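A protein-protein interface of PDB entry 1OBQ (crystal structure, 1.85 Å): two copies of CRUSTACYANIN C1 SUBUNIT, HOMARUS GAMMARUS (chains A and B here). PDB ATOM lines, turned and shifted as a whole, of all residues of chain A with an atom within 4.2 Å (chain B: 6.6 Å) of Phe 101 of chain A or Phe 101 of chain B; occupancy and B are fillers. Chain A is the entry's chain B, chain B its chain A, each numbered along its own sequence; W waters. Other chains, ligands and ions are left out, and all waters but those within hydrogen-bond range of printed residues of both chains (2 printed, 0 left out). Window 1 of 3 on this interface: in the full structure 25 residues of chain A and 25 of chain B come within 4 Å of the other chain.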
ATOM      1  N   TYR A  45      31.142 -28.750 -17.045  1.00  0.00           N
ATOM      2  CA  TYR A  45      30.581 -29.713 -18.004  1.00  0.00           C
ATOM      3  C   TYR A  45      31.456 -29.899 -19.252  1.00  0.00           C
ATOM      4  O   TYR A  45      31.221 -30.769 -20.139  1.00  0.00           O
ATOM      5  CB  TYR A  45      29.237 -29.178 -18.465  1.00  0.00           C
ATOM      6  CG  TYR A  45      28.311 -28.861 -17.281  1.00  0.00           C
ATOM      7  CD1 TYR A  45      27.686 -29.880 -16.594  1.00  0.00           C
ATOM      8  CD2 TYR A  45      27.957 -27.564 -16.961  1.00  0.00           C
ATOM      9  CE1 TYR A  45      26.760 -29.618 -15.584  1.00  0.00           C
ATOM     10  CE2 TYR A  45      27.039 -27.258 -15.955  1.00  0.00           C
ATOM     11  CZ  TYR A  45      26.439 -28.288 -15.257  1.00  0.00           C
ATOM     12  OH  TYR A  45      25.565 -27.981 -14.229  1.00  0.00           O
ATOM     13  N   ILE A  95      22.032 -26.250 -27.147  1.00  0.00           N
ATOM     14  CA  ILE A  95      23.285 -26.949 -27.482  1.00  0.00           C
ATOM     15  C   ILE A  95      23.206 -28.246 -26.745  1.00  0.00           C
ATOM     16  O   ILE A  95      22.996 -28.249 -25.498  1.00  0.00           O
ATOM     17  CB  ILE A  95      24.533 -26.066 -27.192  1.00  0.00           C
ATOM     18  CG1 ILE A  95      25.798 -26.809 -27.579  1.00  0.00           C
ATOM     19  CG2 ILE A  95      24.644 -25.765 -25.770  1.00  0.00           C
ATOM     20  CD1 ILE A  95      26.130 -26.858 -29.019  1.00  0.00           C
ATOM     21  N   ASP A  96      23.446 -29.343 -27.410  1.00  0.00           N
ATOM     22  CA  ASP A  96      23.187 -30.674 -26.855  1.00  0.00           C
ATOM     23  C   ASP A  96      24.335 -31.517 -27.213  1.00  0.00           C
ATOM     24  O   ASP A  96      24.740 -31.547 -28.345  1.00  0.00           O
ATOM     25  CB  ASP A  96      21.865 -31.092 -27.499  1.00  0.00           C
ATOM     26  CG  ASP A  96      21.241 -32.353 -26.918  1.00  0.00           C
ATOM     27  OD1 ASP A  96      21.903 -33.007 -26.136  1.00  0.00           O
ATOM     28  OD2 ASP A  96      20.088 -32.673 -27.181  1.00  0.00           O
ATOM     29  N   TYR A  97      24.927 -32.181 -26.223  1.00  0.00           N
ATOM     30  CA  TYR A  97      26.033 -33.053 -26.447  1.00  0.00           C
ATOM     31  C   TYR A  97      25.766 -34.471 -26.030  1.00  0.00           C
ATOM     32  O   TYR A  97      25.115 -34.680 -24.993  1.00  0.00           O
ATOM     33  CB  TYR A  97      27.240 -32.547 -25.723  1.00  0.00           C
ATOM     34  CG  TYR A  97      28.042 -31.590 -26.551  1.00  0.00           C
ATOM     35  CD1 TYR A  97      27.563 -30.335 -26.818  1.00  0.00           C
ATOM     36  CD2 TYR A  97      29.222 -31.947 -27.150  1.00  0.00           C
ATOM     37  CE1 TYR A  97      28.276 -29.453 -27.617  1.00  0.00           C
ATOM     38  CE2 TYR A  97      29.927 -31.082 -27.977  1.00  0.00           C
ATOM     39  CZ  TYR A  97      29.469 -29.835 -28.177  1.00  0.00           C
ATOM     40  OH  TYR A  97      30.204 -28.988 -28.963  1.00  0.00           O
ATOM     41  N   SER A 100      25.445 -36.137 -22.366  1.00  0.00           N
ATOM     42  CA  SER A 100      25.471 -34.985 -21.505  1.00  0.00           C
ATOM     43  C   SER A 100      24.060 -34.477 -21.399  1.00  0.00           C
ATOM     44  O   SER A 100      23.100 -35.249 -21.281  1.00  0.00           O
ATOM     45  CB  SER A 100      26.418 -33.932 -22.062  1.00  0.00           C
ATOM     46  OG  SER A 100      26.581 -32.833 -21.213  1.00  0.00           O
ATOM     47  N   PHE A 101      23.882 -33.186 -21.368  1.00  0.00           N
ATOM     48  CA  PHE A 101      22.570 -32.655 -21.323  1.00  0.00           C
ATOM     49  C   PHE A 101      22.451 -31.539 -22.403  1.00  0.00           C
ATOM     50  O   PHE A 101      23.410 -31.341 -23.131  1.00  0.00           O
ATOM     51  CB  PHE A 101      22.288 -32.225 -19.962  1.00  0.00           C
ATOM     52  CG  PHE A 101      23.051 -31.084 -19.541  1.00  0.00           C
ATOM     53  CD1 PHE A 101      22.480 -29.880 -19.471  1.00  0.00           C
ATOM     54  CD2 PHE A 101      24.357 -31.243 -19.152  1.00  0.00           C
ATOM     55  CE1 PHE A 101      23.216 -28.806 -19.048  1.00  0.00           C
ATOM     56  CE2 PHE A 101      25.103 -30.142 -18.739  1.00  0.00           C
ATOM     57  CZ  PHE A 101      24.522 -28.952 -18.691  1.00  0.00           C
ATOM     58  N   ALA A 102      21.340 -30.832 -22.479  1.00  0.00           N
ATOM     59  CA  ALA A 102      21.193 -29.745 -23.462  1.00  0.00           C
ATOM     60  C   ALA A 102      20.876 -28.484 -22.714  1.00  0.00           C
ATOM     61  O   ALA A 102      20.141 -28.510 -21.667  1.00  0.00           O
ATOM     62  CB  ALA A 102      20.158 -29.990 -24.391  1.00  0.00           C
ATOM     63  N   ALA A 103      21.485 -27.402 -23.168  1.00  0.00           N
ATOM     64  CA  ALA A 103      21.335 -26.142 -22.516  1.00  0.00           C
ATOM     65  C   ALA A 103      21.003 -25.019 -23.515  1.00  0.00           C
ATOM     66  O   ALA A 103      21.220 -25.163 -24.699  1.00  0.00           O
ATOM     67  CB  ALA A 103      22.566 -25.843 -21.828  1.00  0.00           C
ATOM     68  N   ILE A 122      21.276 -20.742 -16.563  1.00  0.00           N
ATOM     69  CA  ILE A 122      20.279 -21.590 -15.960  1.00  0.00           C
ATOM     70  C   ILE A 122      19.968 -21.034 -14.574  1.00  0.00           C
ATOM     71  O   ILE A 122      20.891 -20.688 -13.841  1.00  0.00           O
ATOM     72  CB  ILE A 122      20.867 -22.996 -15.870  1.00  0.00           C
ATOM     73  CG1 ILE A 122      20.141 -23.891 -14.926  1.00  0.00           C
ATOM     74  CG2 ILE A 122      21.906 -23.003 -15.084  1.00  0.00           C
ATOM     75  CD1 ILE A 122      18.788 -23.974 -15.370  1.00  0.00           C
ATOM     76  N   ASN B  43      16.787 -31.068  -5.258  1.00  0.00           N
ATOM     77  CA  ASN B  43      16.886 -30.762  -6.676  1.00  0.00           C
ATOM     78  C   ASN B  43      16.765 -29.231  -6.853  1.00  0.00           C
ATOM     79  O   ASN B  43      15.720 -28.711  -6.637  1.00  0.00           O
ATOM     80  CB  ASN B  43      15.730 -31.408  -7.496  1.00  0.00           C
ATOM     81  CG  ASN B  43      15.845 -31.195  -9.040  1.00  0.00           C
ATOM     82  OD1 ASN B  43      16.192 -30.100  -9.517  1.00  0.00           O
ATOM     83  ND2 ASN B  43      15.487 -32.231  -9.811  1.00  0.00           N
ATOM     84  N   TYR B  45      16.732 -27.361  -9.451  1.00  0.00           N
ATOM     85  CA  TYR B  45      16.115 -26.951 -10.684  1.00  0.00           C
ATOM     86  C   TYR B  45      14.574 -27.008 -10.682  1.00  0.00           C
ATOM     87  O   TYR B  45      13.924 -26.524 -11.606  1.00  0.00           O
ATOM     88  CB  TYR B  45      16.585 -27.820 -11.766  1.00  0.00           C
ATOM     89  CG  TYR B  45      18.107 -27.881 -11.833  1.00  0.00           C
ATOM     90  CD1 TYR B  45      18.824 -26.783 -12.244  1.00  0.00           C
ATOM     91  CD2 TYR B  45      18.790 -29.015 -11.542  1.00  0.00           C
ATOM     92  CE1 TYR B  45      20.182 -26.803 -12.325  1.00  0.00           C
ATOM     93  CE2 TYR B  45      20.149 -29.047 -11.603  1.00  0.00           C
ATOM     94  CZ  TYR B  45      20.858 -27.953 -12.018  1.00  0.00           C
ATOM     95  OH  TYR B  45      22.276 -27.929 -12.154  1.00  0.00           O
ATOM     96  N   ARG B  79       4.259 -25.088 -15.488  1.00  0.00           N
ATOM     97  CA  ARG B  79       5.394 -25.220 -16.403  1.00  0.00           C
ATOM     98  C   ARG B  79       5.080 -26.209 -17.521  1.00  0.00           C
ATOM     99  O   ARG B  79       4.501 -27.319 -17.251  1.00  0.00           O
ATOM    100  CB  ARG B  79       6.599 -25.744 -15.701  1.00  0.00           C
ATOM    101  CG  ARG B  79       6.810 -25.132 -14.359  1.00  0.00           C
ATOM    102  CD  ARG B  79       8.162 -25.469 -13.794  1.00  0.00           C
ATOM    103  NE  ARG B  79       9.348 -25.158 -14.597  1.00  0.00           N
ATOM    104  CZ  ARG B  79      10.561 -25.674 -14.296  1.00  0.00           C
ATOM    105  NH1 ARG B  79      10.681 -26.545 -13.272  1.00  0.00           N
ATOM    106  NH2 ARG B  79      11.639 -25.321 -14.980  1.00  0.00           N
ATOM    107  N   ILE B  95      14.175 -35.027 -20.844  1.00  0.00           N
ATOM    108  CA  ILE B  95      13.084 -34.268 -20.295  1.00  0.00           C
ATOM    109  C   ILE B  95      13.517 -32.780 -20.457  1.00  0.00           C
ATOM    110  O   ILE B  95      14.667 -32.427 -20.095  1.00  0.00           O
ATOM    111  CB  ILE B  95      12.894 -34.696 -18.827  1.00  0.00           C
ATOM    112  CG1 ILE B  95      11.752 -33.915 -18.179  1.00  0.00           C
ATOM    113  CG2 ILE B  95      14.129 -34.465 -17.931  1.00  0.00           C
ATOM    114  CD1 ILE B  95      10.594 -34.067 -18.891  1.00  0.00           C
ATOM    115  N   ASP B  96      12.657 -31.960 -21.052  1.00  0.00           N
ATOM    116  CA  ASP B  96      12.985 -30.599 -21.421  1.00  0.00           C
ATOM    117  C   ASP B  96      11.816 -29.732 -20.953  1.00  0.00           C
ATOM    118  O   ASP B  96      10.649 -30.061 -21.159  1.00  0.00           O
ATOM    119  CB  ASP B  96      13.073 -30.663 -22.963  1.00  0.00           C
ATOM    120  CG  ASP B  96      13.684 -29.398 -23.595  1.00  0.00           C
ATOM    121  OD1 ASP B  96      13.960 -28.451 -22.884  1.00  0.00           O
ATOM    122  OD2 ASP B  96      14.008 -29.481 -24.812  1.00  0.00           O
ATOM    123  N   TYR B  97      12.128 -28.648 -20.273  1.00  0.00           N
ATOM    124  CA  TYR B  97      11.150 -27.705 -19.869  1.00  0.00           C
ATOM    125  C   TYR B  97      11.466 -26.313 -20.464  1.00  0.00           C
ATOM    126  O   TYR B  97      12.628 -25.872 -20.439  1.00  0.00           O
ATOM    127  CB  TYR B  97      11.113 -27.656 -18.384  1.00  0.00           C
ATOM    128  CG  TYR B  97      10.192 -28.736 -17.708  1.00  0.00           C
ATOM    129  CD1 TYR B  97      10.608 -30.001 -17.506  1.00  0.00           C
ATOM    130  CD2 TYR B  97       8.881 -28.416 -17.381  1.00  0.00           C
ATOM    131  CE1 TYR B  97       9.762 -30.962 -16.962  1.00  0.00           C
ATOM    132  CE2 TYR B  97       8.028 -29.300 -16.791  1.00  0.00           C
ATOM    133  CZ  TYR B  97       8.445 -30.616 -16.607  1.00  0.00           C
ATOM    134  OH  TYR B  97       7.644 -31.557 -15.991  1.00  0.00           O
ATOM    135  N   GLU B  98      10.378 -25.628 -20.698  1.00  0.00           N
ATOM    136  CA  GLU B  98      10.339 -24.315 -21.265  1.00  0.00           C
ATOM    137  C   GLU B  98      11.097 -23.381 -20.357  1.00  0.00           C
ATOM    138  O   GLU B  98      10.961 -23.425 -19.162  1.00  0.00           O
ATOM    139  CB  GLU B  98       8.905 -23.917 -21.333  1.00  0.00           C
ATOM    140  CG  GLU B  98       8.571 -23.002 -22.458  1.00  0.00           C
ATOM    141  CD  GLU B  98       7.129 -22.494 -22.385  1.00  0.00           C
ATOM    142  OE1 GLU B  98       6.475 -22.670 -21.322  1.00  0.00           O
ATOM    143  OE2 GLU B  98       6.723 -21.881 -23.397  1.00  0.00           O
ATOM    144  N   ASN B  99      12.025 -22.651 -20.934  1.00  0.00           N
ATOM    145  CA  ASN B  99      12.845 -21.697 -20.219  1.00  0.00           C
ATOM    146  C   ASN B  99      13.744 -22.354 -19.228  1.00  0.00           C
ATOM    147  O   ASN B  99      14.144 -21.730 -18.203  1.00  0.00           O
ATOM    148  CB  ASN B  99      11.962 -20.691 -19.477  1.00  0.00           C
ATOM    149  CG  ASN B  99      11.116 -19.845 -20.437  1.00  0.00           C
ATOM    150  OD1 ASN B  99       9.886 -19.736 -20.263  1.00  0.00           O
ATOM    151  ND2 ASN B  99      11.774 -19.258 -21.472  1.00  0.00           N
ATOM    152  N   SER B 100      14.116 -23.594 -19.494  1.00  0.00           N
ATOM    153  CA  SER B 100      15.008 -24.266 -18.608  1.00  0.00           C
ATOM    154  C   SER B 100      15.989 -25.018 -19.458  1.00  0.00           C
ATOM    155  O   SER B 100      16.501 -24.487 -20.408  1.00  0.00           O
ATOM    156  CB  SER B 100      14.231 -25.135 -17.609  1.00  0.00           C
ATOM    157  OG  SER B 100      15.119 -25.766 -16.754  1.00  0.00           O
ATOM    158  N   PHE B 101      16.305 -26.234 -19.125  1.00  0.00           N
ATOM    159  CA  PHE B 101      17.295 -26.956 -19.910  1.00  0.00           C
ATOM    160  C   PHE B 101      16.737 -28.392 -20.062  1.00  0.00           C
ATOM    161  O   PHE B 101      15.655 -28.673 -19.522  1.00  0.00           O
ATOM    162  CB  PHE B 101      18.629 -26.987 -19.233  1.00  0.00           C
ATOM    163  CG  PHE B 101      18.646 -27.569 -17.886  1.00  0.00           C
ATOM    164  CD1 PHE B 101      19.136 -28.871 -17.716  1.00  0.00           C
ATOM    165  CD2 PHE B 101      18.323 -26.796 -16.762  1.00  0.00           C
ATOM    166  CE1 PHE B 101      19.249 -29.439 -16.440  1.00  0.00           C
ATOM    167  CE2 PHE B 101      18.401 -27.342 -15.478  1.00  0.00           C
ATOM    168  CZ  PHE B 101      18.855 -28.659 -15.297  1.00  0.00           C
ATOM    169  N   ALA B 102      17.381 -29.206 -20.834  1.00  0.00           N
ATOM    170  CA  ALA B 102      16.983 -30.608 -20.945  1.00  0.00           C
ATOM    171  C   ALA B 102      18.018 -31.546 -20.360  1.00  0.00           C
ATOM    172  O   ALA B 102      19.233 -31.286 -20.481  1.00  0.00           O
ATOM    173  CB  ALA B 102      16.713 -30.978 -22.380  1.00  0.00           C
ATOM    174  N   ALA B 103      17.541 -32.667 -19.746  1.00  0.00           N
ATOM    175  CA  ALA B 103      18.394 -33.617 -19.096  1.00  0.00           C
ATOM    176  C   ALA B 103      17.924 -35.066 -19.430  1.00  0.00           C
ATOM    177  O   ALA B 103      16.777 -35.263 -19.793  1.00  0.00           O
ATOM    178  CB  ALA B 103      18.412 -33.376 -17.615  1.00  0.00           C
ATOM    179  N   PRO B 104      18.839 -35.998 -19.381  1.00  0.00           N
ATOM    180  CA  PRO B 104      18.538 -37.380 -19.671  1.00  0.00           C
ATOM    181  C   PRO B 104      17.637 -37.879 -18.548  1.00  0.00           C
ATOM    182  O   PRO B 104      17.709 -37.441 -17.406  1.00  0.00           O
ATOM    183  CB  PRO B 104      19.880 -38.085 -19.659  1.00  0.00           C
ATOM    184  CG  PRO B 104      20.836 -37.173 -19.057  1.00  0.00           C
ATOM    185  CD  PRO B 104      20.247 -35.816 -18.993  1.00  0.00           C
ATOM    186  N   ILE B 122      24.195 -36.610 -14.328  1.00  0.00           N
ATOM    187  CA  ILE B 122      25.148 -35.838 -15.119  1.00  0.00           C
ATOM    188  C   ILE B 122      26.593 -35.925 -14.515  1.00  0.00           C
ATOM    189  O   ILE B 122      26.754 -35.806 -13.284  1.00  0.00           O
ATOM    190  CB  ILE B 122      24.681 -34.408 -15.201  1.00  0.00           C
ATOM    191  CG1 ILE B 122      25.597 -33.512 -16.002  1.00  0.00           C
ATOM    192  CG2 ILE B 122      24.763 -33.678 -13.898  1.00  0.00           C
ATOM    193  CD1 ILE B 122      25.455 -33.597 -17.434  1.00  0.00           C
ATOM    194  N   ASP B 123      27.561 -36.258 -15.372  1.00  0.00           N
ATOM    195  CA  ASP B 123      28.975 -36.246 -14.998  1.00  0.00           C
ATOM    196  C   ASP B 123      29.591 -34.888 -15.134  1.00  0.00           C
ATOM    197  O   ASP B 123      29.318 -34.172 -16.110  1.00  0.00           O
ATOM    198  CB  ASP B 123      29.689 -37.209 -15.822  1.00  0.00           C
ATOM    199  CG  ASP B 123      29.436 -38.611 -15.405  1.00  0.00           C
ATOM    200  OD1 ASP B 123      29.521 -39.015 -14.246  1.00  0.00           O
ATOM    201  OD2 ASP B 123      29.174 -39.482 -16.227  1.00  0.00           O
ATOM    202  N   PHE B 132      19.575 -36.954  -9.718  1.00  0.00           N
ATOM    203  CA  PHE B 132      18.253 -36.504  -9.323  1.00  0.00           C
ATOM    204  C   PHE B 132      17.311 -37.697  -9.561  1.00  0.00           C
ATOM    205  O   PHE B 132      17.311 -38.292 -10.634  1.00  0.00           O
ATOM    206  CB  PHE B 132      17.922 -35.318 -10.191  1.00  0.00           C
ATOM    207  CG  PHE B 132      19.017 -34.239 -10.148  1.00  0.00           C
ATOM    208  CD1 PHE B 132      19.084 -33.445  -9.083  1.00  0.00           C
ATOM    209  CD2 PHE B 132      19.962 -34.130 -11.140  1.00  0.00           C
ATOM    210  CE1 PHE B 132      20.125 -32.534  -8.947  1.00  0.00           C
ATOM    211  CE2 PHE B 132      20.969 -33.149 -11.036  1.00  0.00           C
ATOM    212  CZ  PHE B 132      20.996 -32.371  -9.981  1.00  0.00           C
HETATM  213  O   HOH W   1      23.732 -26.039 -13.125  1.00  0.00           O
HETATM  214  O   HOH W   2      24.188 -29.771 -12.463  1.00  0.00           O
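The side-chain amide oxygen (OD1) of Asn 43 of chain B is in hydrogen-bond range of the backbone NH (N) of Tyr 45 of chain B (2.8 Å).
Of the 16 printed residues of chain B, 5 touch a printed residue of chain A. Hydrophobic or aromatic side chains of chain B that line the printed part of chain A: Tyr 45, Phe 101, Pro 104 and Ile 122. Among the printed residues, 9 pairs touch across the chains.
Phe 101 of chain A touches just these residues of chain B: Phe 101, Ala 102 and Ile 122. Of the printed residues of chain B, Ile 122 of chain A touches Tyr 45 and Phe 101. Of chain A, only Phe 101 (3.9 Å), Ala 102 (3.2 Å) and Ile 122 (3.2 Å) come within 4 Å of Phe 101 of chain B. Printed residues of chain A within 4 Å of Pro 104 of chain B: Ser 100. The nearest printed residue of chain B that does not touch Phe 101 of chain A is Ala 103 of chain B (4.2 Å). The nearest printed residue of chain A that does not touch Phe 101 of chain B is Ala 103 of chain A (4.3 Å). The nearest printed residue of chain B that does not touch Ala 102 of chain A is Ala 103 of chain B (5.0 Å).
Water W1 lies within hydrogen-bond range of OH of Tyr 45 of chain B and OH of Tyr 45 of chain A. Water W2 bridges OH of Tyr 45 of chain B and OH of Tyr 45 of chain A.
Among the printed residues, merely in contact across the chains: Tyr 45 of chain A with Tyr 45 of chain B, Ser 100 of chain A with Pro 104 of chain B, Phe 101 of chain A with Phe 101 of chain B, Phe 101 of chain A with Ala 102 of chain B, Phe 101 of chain A with Ile 122 of chain B, Ala 102 of chain A with Phe 101 of chain B, Ile 122 of chain A with Tyr 45 of chain B and Ile 122 of chain A with Phe 101 of chain B.
Tyr 45 of chain A touches its own counterpart, Tyr 45 of chain B. Phe 101 of chain B touches its own counterpart, Phe 101 of chain A. Phe 101 of chain A touches Ala 102 of chain B, and with the chains exchanged Ala 102 of chain A touches Phe 101 of chain B. Ile 122 of chain A touches Tyr 45 of chain B, but with the chains exchanged Tyr 45 of chain A does not touch Ile 122 of chain B (4.1 Å). 9 positions are printed for both chains. Of the 9 pairs that touch across the chains among the printed residues, 7 have their exchanged pair printed and touching as well.
The backbone carbonyl oxygen of Ala 102 of chain B lies within hydrogen-bond range of the backbone NH of Ala 102 of chain A (2.9 Å).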
